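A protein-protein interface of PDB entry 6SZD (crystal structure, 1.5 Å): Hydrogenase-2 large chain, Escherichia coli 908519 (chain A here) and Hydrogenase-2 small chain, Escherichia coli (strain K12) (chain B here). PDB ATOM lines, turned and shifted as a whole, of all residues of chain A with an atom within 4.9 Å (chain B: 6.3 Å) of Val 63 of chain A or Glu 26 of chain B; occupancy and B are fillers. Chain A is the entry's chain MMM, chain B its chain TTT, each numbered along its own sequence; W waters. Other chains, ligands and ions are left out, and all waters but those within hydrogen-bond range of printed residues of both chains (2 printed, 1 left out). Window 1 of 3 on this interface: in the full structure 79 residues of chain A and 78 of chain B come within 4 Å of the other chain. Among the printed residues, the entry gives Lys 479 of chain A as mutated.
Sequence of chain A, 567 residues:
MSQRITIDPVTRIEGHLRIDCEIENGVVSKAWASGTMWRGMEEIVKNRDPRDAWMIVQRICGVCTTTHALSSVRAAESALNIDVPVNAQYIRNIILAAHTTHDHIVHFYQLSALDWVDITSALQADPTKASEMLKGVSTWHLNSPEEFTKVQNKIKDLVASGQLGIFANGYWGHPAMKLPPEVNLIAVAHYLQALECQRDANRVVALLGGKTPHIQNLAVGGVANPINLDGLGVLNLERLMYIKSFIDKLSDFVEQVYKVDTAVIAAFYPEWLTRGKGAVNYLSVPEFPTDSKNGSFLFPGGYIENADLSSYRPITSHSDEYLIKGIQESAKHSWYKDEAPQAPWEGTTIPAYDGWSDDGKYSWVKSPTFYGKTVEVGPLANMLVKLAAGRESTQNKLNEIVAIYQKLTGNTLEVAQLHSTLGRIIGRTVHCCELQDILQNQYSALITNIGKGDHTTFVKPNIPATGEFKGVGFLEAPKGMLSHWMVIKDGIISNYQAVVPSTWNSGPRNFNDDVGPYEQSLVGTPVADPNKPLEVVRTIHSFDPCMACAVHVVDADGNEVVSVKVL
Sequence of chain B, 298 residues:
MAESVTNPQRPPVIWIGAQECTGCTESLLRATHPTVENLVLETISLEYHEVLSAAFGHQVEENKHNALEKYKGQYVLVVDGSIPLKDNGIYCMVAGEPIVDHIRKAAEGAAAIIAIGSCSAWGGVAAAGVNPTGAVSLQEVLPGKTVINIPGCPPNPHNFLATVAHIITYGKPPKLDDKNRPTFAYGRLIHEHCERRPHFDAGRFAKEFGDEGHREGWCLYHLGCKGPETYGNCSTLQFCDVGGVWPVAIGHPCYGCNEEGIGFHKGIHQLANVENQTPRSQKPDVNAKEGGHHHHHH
The side-chain hydroxyl (OG1) of Thr 22 of chain B sits at hydrogen-bond distance from the side-chain carboxylate (OE2) of Glu 14 of chain A, 2.5 Å away.
OE2 of Glu 14 of chain A sits close to O of Cys 21 of chain B (3.4 Å).
The backbone NH (N) of Gly 62 of chain A is in hydrogen-bond range of the backbone carbonyl oxygen (O) of Cys 21 of chain B (2.8 Å).
NE2 of His 99 of chain A sits close to O of Val 63 of chain A (3.2 Å).
O of Cys 24 of chain B lies within hydrogen-bond range of OG of Ser 27 of chain B (2.7 Å).
The side-chain sulfur of Cys 21 of chain B sits close to the backbone NH of Gly 23 of chain B (3.3 Å).
NH1 of Arg 30 of chain B is in salt-bridge range of OE1 of Glu 26 of chain B (2.9 Å).
SG of Cys 61 of chain A sits close to N of Val 63 of chain A, 3.4 Å away.
O of Cys 21 of chain B touches C of Cys 61 of chain A, at 3.7 Å.
Gly 62 of chain A touches Gly 23 of chain B.
O of Gly 62 of chain A touches CG of Glu 26 of chain B, 3.5 Å away.
N of Val 63 of chain A touches O of Cys 21 of chain B (3.9 Å).
Val 63 of chain A touches Thr 22 of chain B (CG2 to CG2, 3.5 Å).
CE1 of His 102 of chain A touches OE1 of Glu 26 of chain B, at 3.4 Å.
Arg 30 of chain B touches His 102 of chain A (NH1 to CE1, 3.6 Å).
Pro 213 of chain A touches Gly 23 of chain B.
CB of Glu 26 of chain B touches CG of Pro 213 of chain A, at 3.8 Å.
Ser 27 of chain B touches Pro 213 of chain A (N to CG, 3.9 Å).
Val 63 of chain A touches just these residues of chain B: Cys 21 (3.9 Å), Thr 22 (3.5 Å) and Glu 26 (3.5 Å).
Glu 26 of chain B touches just these residues of chain A: Gly 62 (3.5 Å), Val 63 (3.5 Å), His 102 (3.4 Å) and Pro 213 (3.8 Å).
Of the printed residues of chain A, Arg 30 of chain B touches His 102 and Pro 213.
Of the printed residues of chain A, Ser 27 of chain B touches Pro 213.
Printed residues of chain A within 4 Å of Thr 22 of chain B: Glu 14 and Val 63.
Printed residues of chain B within 4 Å of Cys 61 of chain A: Cys 21 (3.7 Å).
Printed residues of chain A within 4 Å of Pro 154 of chain B: Pro 213 (3.4 Å).
Val 51 of chain B touches none of the printed residues of chain A.
The nearest printed residue of chain A that does not touch Cys 21 of chain B is Cys 64 of chain A (6.1 Å).
Of the 11 printed residues of chain A, 6 touch a printed residue of chain B.
Hydrophobic or aromatic side chains of chain A that line the printed part of chain B: Val 63, His 102 and Pro 213.
Printed residues of chain B that touch a printed residue of chain A: Cys 21, Thr 22, Gly 23, Glu 26, Ser 27, Arg 30 and Pro 154.
Water W2 lies within hydrogen-bond range of the side-chain carboxylate (OE2) of Glu 26 of chain B (2.6 Å) and a ring nitrogen (NE2) of His 102 of chain A (3.0 Å).
Water W1 bridges a ring nitrogen (ND1) of His 99 of chain A (2.8 Å) and the guanidinium group (NH2) of Arg 30 of chain B (3.5 Å).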
ATOM      1  N   GLU A  14      27.246  12.548  14.224  1.00  0.00           N
ATOM      2  CA  GLU A  14      26.405  12.674  13.013  1.00  0.00           C
ATOM      3  C   GLU A  14      26.804  13.916  12.218  1.00  0.00           C
ATOM      4  O   GLU A  14      26.810  15.012  12.804  1.00  0.00           O
ATOM      5  CB  GLU A  14      24.922  12.718  13.388  1.00  0.00           C
ATOM      6  CG  GLU A  14      24.014  12.563  12.173  1.00  0.00           C
ATOM      7  CD  GLU A  14      24.067  13.665  11.124  1.00  0.00           C
ATOM      8  OE1 GLU A  14      24.247  14.856  11.559  1.00  0.00           O
ATOM      9  OE2 GLU A  14      23.910  13.375   9.877  1.00  0.00           O
ATOM     10  N   CYS A  61      17.150  14.387  10.389  1.00  0.00           N
ATOM     11  CA  CYS A  61      18.174  13.492  10.951  1.00  0.00           C
ATOM     12  C   CYS A  61      17.695  12.051  11.044  1.00  0.00           C
ATOM     13  O   CYS A  61      16.552  11.839  11.496  1.00  0.00           O
ATOM     14  CB  CYS A  61      18.574  14.019  12.309  1.00  0.00           C
ATOM     15  SG  CYS A  61      19.972  13.158  13.058  1.00  0.00           S
ATOM     16  N   GLY A  62      18.581  11.118  10.695  1.00  0.00           N
ATOM     17  CA  GLY A  62      18.334   9.673  10.827  1.00  0.00           C
ATOM     18  C   GLY A  62      18.947   9.058  12.052  1.00  0.00           C
ATOM     19  O   GLY A  62      18.641   7.891  12.342  1.00  0.00           O
ATOM     20  N   VAL A  63      19.849   9.734  12.741  1.00  0.00           N
ATOM     21  CA  VAL A  63      20.338   9.266  14.046  1.00  0.00           C
ATOM     22  C   VAL A  63      19.254   9.551  15.077  1.00  0.00           C
ATOM     23  O   VAL A  63      18.727   8.596  15.656  1.00  0.00           O
ATOM     24  CB  VAL A  63      21.679   9.932  14.410  1.00  0.00           C
ATOM     25  CG1 VAL A  63      22.107   9.501  15.800  1.00  0.00           C
ATOM     26  CG2 VAL A  63      22.747   9.582  13.381  1.00  0.00           C
ATOM     27  N   CYS A  64      18.828  10.802  15.194  1.00  0.00           N
ATOM     28  CA  CYS A  64      17.668  11.166  16.064  1.00  0.00           C
ATOM     29  C   CYS A  64      16.418  11.083  15.208  1.00  0.00           C
ATOM     30  O   CYS A  64      15.563  11.988  15.218  1.00  0.00           O
ATOM     31  CB  CYS A  64      17.861  12.470  16.805  1.00  0.00           C
ATOM     32  SG  CYS A  64      18.049  13.914  15.743  1.00  0.00           S
ATOM     33  N   THR A  65      16.267   9.949  14.515  1.00  0.00           N
ATOM     34  CA  THR A  65      14.979   9.651  13.864  1.00  0.00           C
ATOM     35  C   THR A  65      13.907   9.639  14.966  1.00  0.00           C
ATOM     36  O   THR A  65      14.228   9.567  16.160  1.00  0.00           O
ATOM     37  CB  THR A  65      15.106   8.373  13.008  1.00  0.00           C
ATOM     38  OG1 THR A  65      13.919   8.248  12.238  1.00  0.00           O
ATOM     39  CG2 THR A  65      15.361   7.148  13.858  1.00  0.00           C
ATOM     40  N   HIS A  99      13.638   4.682  21.221  1.00  0.00           N
ATOM     41  CA  HIS A  99      14.591   5.307  20.274  1.00  0.00           C
ATOM     42  C   HIS A  99      15.753   5.891  21.085  1.00  0.00           C
ATOM     43  O   HIS A  99      16.920   5.665  20.730  1.00  0.00           O
ATOM     44  CB  HIS A  99      13.948   6.406  19.423  1.00  0.00           C
ATOM     45  CG  HIS A  99      15.045   7.087  18.697  1.00  0.00           C
ATOM     46  ND1 HIS A  99      15.605   6.538  17.595  1.00  0.00           N
ATOM     47  CD2 HIS A  99      15.839   8.111  19.069  1.00  0.00           C
ATOM     48  CE1 HIS A  99      16.689   7.240  17.268  1.00  0.00           C
ATOM     49  NE2 HIS A  99      16.844   8.197  18.151  1.00  0.00           N
ATOM     50  N   HIS A 102      18.323   3.354  22.304  1.00  0.00           N
ATOM     51  CA  HIS A 102      19.261   3.027  21.194  1.00  0.00           C
ATOM     52  C   HIS A 102      20.272   4.161  21.023  1.00  0.00           C
ATOM     53  O   HIS A 102      21.482   3.911  20.861  1.00  0.00           O
ATOM     54  CB  HIS A 102      18.480   2.756  19.890  1.00  0.00           C
ATOM     55  CG  HIS A 102      19.140   3.261  18.661  1.00  0.00           C
ATOM     56  ND1 HIS A 102      20.062   2.516  17.928  1.00  0.00           N
ATOM     57  CD2 HIS A 102      18.946   4.399  17.979  1.00  0.00           C
ATOM     58  CE1 HIS A 102      20.461   3.260  16.892  1.00  0.00           C
ATOM     59  NE2 HIS A 102      19.787   4.420  16.914  1.00  0.00           N
ATOM     60  N   ASP A 103      19.793   5.378  21.023  1.00  0.00           N
ATOM     61  CA  ASP A 103      20.618   6.547  20.638  1.00  0.00           C
ATOM     62  C   ASP A 103      21.749   6.700  21.679  1.00  0.00           C
ATOM     63  O   ASP A 103      22.926   6.811  21.299  1.00  0.00           O
ATOM     64  CB  ASP A 103      19.650   7.719  20.575  1.00  0.00           C
ATOM     65  CG  ASP A 103      20.120   8.918  19.805  1.00  0.00           C
ATOM     66  OD1 ASP A 103      21.271   9.352  20.101  1.00  0.00           O
ATOM     67  OD2 ASP A 103      19.315   9.488  19.016  1.00  0.00           O
ATOM     68  N   PRO A 213      15.241   3.113  10.625  1.00  0.00           N
ATOM     69  CA  PRO A 213      14.959   4.543  10.765  1.00  0.00           C
ATOM     70  C   PRO A 213      13.728   5.055  10.012  1.00  0.00           C
ATOM     71  O   PRO A 213      13.296   4.447   9.020  1.00  0.00           O
ATOM     72  CB  PRO A 213      16.186   5.201  10.099  1.00  0.00           C
ATOM     73  CG  PRO A 213      17.266   4.145  10.163  1.00  0.00           C
ATOM     74  CD  PRO A 213      16.545   2.839   9.993  1.00  0.00           C
ATOM     75  N   LYS A 479      19.557  14.591  22.353  1.00  0.00           N
ATOM     76  CA  LYS A 479      20.578  15.676  22.440  1.00  0.00           C
ATOM     77  C   LYS A 479      20.055  16.928  23.131  1.00  0.00           C
ATOM     78  O   LYS A 479      20.903  17.815  23.375  1.00  0.00           O
ATOM     79  CB  LYS A 479      21.090  16.057  21.045  1.00  0.00           C
ATOM     80  CG  LYS A 479      22.350  15.297  20.609  1.00  0.00           C
ATOM     81  CD  LYS A 479      22.177  14.256  19.505  1.00  0.00           C
ATOM     82  CE  LYS A 479      21.528  12.983  20.014  1.00  0.00           C
ATOM     83  NZ  LYS A 479      22.099  11.803  19.327  1.00  0.00           N
ATOM     84  N   CYS B  21      21.320  12.458   6.042  1.00  0.00           N
ATOM     85  CA  CYS B  21      20.751  12.593   7.409  1.00  0.00           C
ATOM     86  C   CYS B  21      21.335  11.517   8.339  1.00  0.00           C
ATOM     87  O   CYS B  21      21.051  11.520   9.542  1.00  0.00           O
ATOM     88  CB  CYS B  21      19.235  12.530   7.397  1.00  0.00           C
ATOM     89  SG  CYS B  21      18.578  10.832   7.267  1.00  0.00           S
ATOM     90  N   THR B  22      22.085  10.550   7.782  1.00  0.00           N
ATOM     91  CA  THR B  22      22.762   9.419   8.466  1.00  0.00           C
ATOM     92  C   THR B  22      21.797   8.228   8.609  1.00  0.00           C
ATOM     93  O   THR B  22      22.222   7.162   9.011  1.00  0.00           O
ATOM     94  CB  THR B  22      23.470   9.821   9.775  1.00  0.00           C
ATOM     95  OG1 THR B  22      24.258  10.967   9.412  1.00  0.00           O
ATOM     96  CG2 THR B  22      24.365   8.745  10.352  1.00  0.00           C
ATOM     97  N   GLY B  23      20.526   8.386   8.240  1.00  0.00           N
ATOM     98  CA  GLY B  23      19.578   7.260   8.330  1.00  0.00           C
ATOM     99  C   GLY B  23      19.992   6.060   7.490  1.00  0.00           C
ATOM    100  O   GLY B  23      19.708   4.937   7.882  1.00  0.00           O
ATOM    101  N   CYS B  24      20.688   6.258   6.381  1.00  0.00           N
ATOM    102  CA  CYS B  24      21.134   5.140   5.508  1.00  0.00           C
ATOM    103  C   CYS B  24      22.244   4.347   6.193  1.00  0.00           C
ATOM    104  O   CYS B  24      22.211   3.119   6.181  1.00  0.00           O
ATOM    105  CB  CYS B  24      21.539   5.652   4.124  1.00  0.00           C
ATOM    106  SG  CYS B  24      20.137   6.175   3.109  1.00  0.00           S
ATOM    107  N   THR B  25      23.203   4.999   6.864  1.00  0.00           N
ATOM    108  CA  THR B  25      24.150   4.287   7.766  1.00  0.00           C
ATOM    109  C   THR B  25      23.414   3.626   8.931  1.00  0.00           C
ATOM    110  O   THR B  25      23.679   2.449   9.255  1.00  0.00           O
ATOM    111  CB  THR B  25      25.204   5.233   8.345  1.00  0.00           C
ATOM    112  OG1 THR B  25      26.021   5.615   7.223  1.00  0.00           O
ATOM    113  CG2 THR B  25      26.010   4.553   9.412  1.00  0.00           C
ATOM    114  N   GLU B  26      22.480   4.349   9.547  1.00  0.00           N
ATOM    115  CA  GLU B  26      21.760   3.804  10.722  1.00  0.00           C
ATOM    116  C   GLU B  26      20.967   2.553  10.338  1.00  0.00           C
ATOM    117  O   GLU B  26      20.756   1.685  11.240  1.00  0.00           O
ATOM    118  CB  GLU B  26      20.809   4.861  11.260  1.00  0.00           C
ATOM    119  CG  GLU B  26      21.520   5.858  12.113  1.00  0.00           C
ATOM    120  CD  GLU B  26      21.894   5.417  13.507  1.00  0.00           C
ATOM    121  OE1 GLU B  26      21.609   4.287  13.890  1.00  0.00           O
ATOM    122  OE2 GLU B  26      22.513   6.209  14.246  1.00  0.00           O
ATOM    123  N   SER B  27      20.547   2.421   9.098  1.00  0.00           N
ATOM    124  CA  SER B  27      19.839   1.188   8.653  1.00  0.00           C
ATOM    125  C   SER B  27      20.729  -0.008   8.987  1.00  0.00           C
ATOM    126  O   SER B  27      20.215  -1.082   9.354  1.00  0.00           O
ATOM    127  CB  SER B  27      19.421   1.209   7.203  1.00  0.00           C
ATOM    128  OG  SER B  27      20.509   1.006   6.305  1.00  0.00           O
ATOM    129  N   LEU B  28      22.050   0.136   8.854  1.00  0.00           N
ATOM    130  CA  LEU B  28      22.952  -1.017   9.095  1.00  0.00           C
ATOM    131  C   LEU B  28      22.837  -1.511  10.530  1.00  0.00           C
ATOM    132  O   LEU B  28      23.136  -2.691  10.754  1.00  0.00           O
ATOM    133  CB  LEU B  28      24.401  -0.668   8.779  1.00  0.00           C
ATOM    134  CG  LEU B  28      24.652  -0.179   7.357  1.00  0.00           C
ATOM    135  CD1 LEU B  28      26.124   0.164   7.194  1.00  0.00           C
ATOM    136  CD2 LEU B  28      24.269  -1.217   6.346  1.00  0.00           C
ATOM    137  N   LEU B  29      22.516  -0.641  11.486  1.00  0.00           N
ATOM    138  CA  LEU B  29      22.460  -1.012  12.913  1.00  0.00           C
ATOM    139  C   LEU B  29      21.188  -1.828  13.171  1.00  0.00           C
ATOM    140  O   LEU B  29      21.098  -2.362  14.268  1.00  0.00           O
ATOM    141  CB  LEU B  29      22.542   0.223  13.818  1.00  0.00           C
ATOM    142  CG  LEU B  29      23.985   0.642  14.154  1.00  0.00           C
ATOM    143  CD1 LEU B  29      24.787   1.016  12.926  1.00  0.00           C
ATOM    144  CD2 LEU B  29      23.980   1.766  15.163  1.00  0.00           C
ATOM    145  N   ARG B  30      20.250  -1.925  12.231  1.00  0.00           N
ATOM    146  CA  ARG B  30      19.051  -2.802  12.361  1.00  0.00           C
ATOM    147  C   ARG B  30      19.289  -4.136  11.639  1.00  0.00           C
ATOM    148  O   ARG B  30      18.533  -5.076  11.859  1.00  0.00           O
ATOM    149  CB  ARG B  30      17.812  -2.129  11.763  1.00  0.00           C
ATOM    150  CG  ARG B  30      17.218  -0.976  12.567  1.00  0.00           C
ATOM    151  CD  ARG B  30      18.059   0.281  12.556  1.00  0.00           C
ATOM    152  NE  ARG B  30      17.344   1.468  13.013  1.00  0.00           N
ATOM    153  CZ  ARG B  30      17.932   2.541  13.513  1.00  0.00           C
ATOM    154  NH1 ARG B  30      19.258   2.627  13.523  1.00  0.00           N
ATOM    155  NH2 ARG B  30      17.196   3.571  13.911  1.00  0.00           N
ATOM    156  N   ALA B  31      20.315  -4.242  10.812  1.00  0.00           N
ATOM    157  CA  ALA B  31      20.559  -5.428   9.965  1.00  0.00           C
ATOM    158  C   ALA B  31      20.876  -6.648  10.832  1.00  0.00           C
ATOM    159  O   ALA B  31      21.482  -6.529  11.894  1.00  0.00           O
ATOM    160  CB  ALA B  31      21.687  -5.191   8.985  1.00  0.00           C
ATOM    161  N   VAL B  51      31.249   7.902  10.409  1.00  0.00           N
ATOM    162  CA  VAL B  51      30.418   7.723  11.629  1.00  0.00           C
ATOM    163  C   VAL B  51      31.114   6.815  12.626  1.00  0.00           C
ATOM    164  O   VAL B  51      30.917   7.013  13.829  1.00  0.00           O
ATOM    165  CB  VAL B  51      29.005   7.219  11.264  1.00  0.00           C
ATOM    166  CG1 VAL B  51      28.189   6.847  12.515  1.00  0.00           C
ATOM    167  CG2 VAL B  51      28.279   8.252  10.402  1.00  0.00           C
ATOM    168  N   PRO B 154      15.207   5.291   4.904  1.00  0.00           N
ATOM    169  CA  PRO B 154      16.228   4.588   4.116  1.00  0.00           C
ATOM    170  C   PRO B 154      15.702   3.237   3.632  1.00  0.00           C
ATOM    171  O   PRO B 154      14.696   2.702   4.137  1.00  0.00           O
ATOM    172  CB  PRO B 154      17.325   4.347   5.143  1.00  0.00           C
ATOM    173  CG  PRO B 154      16.529   4.129   6.457  1.00  0.00           C
ATOM    174  CD  PRO B 154      15.304   5.010   6.352  1.00  0.00           C
HETATM  175  O   HOH W   1      14.631   4.350  16.146  1.00  0.00           O
HETATM  176  O   HOH W   2      22.481   5.834  16.798  1.00  0.00           O
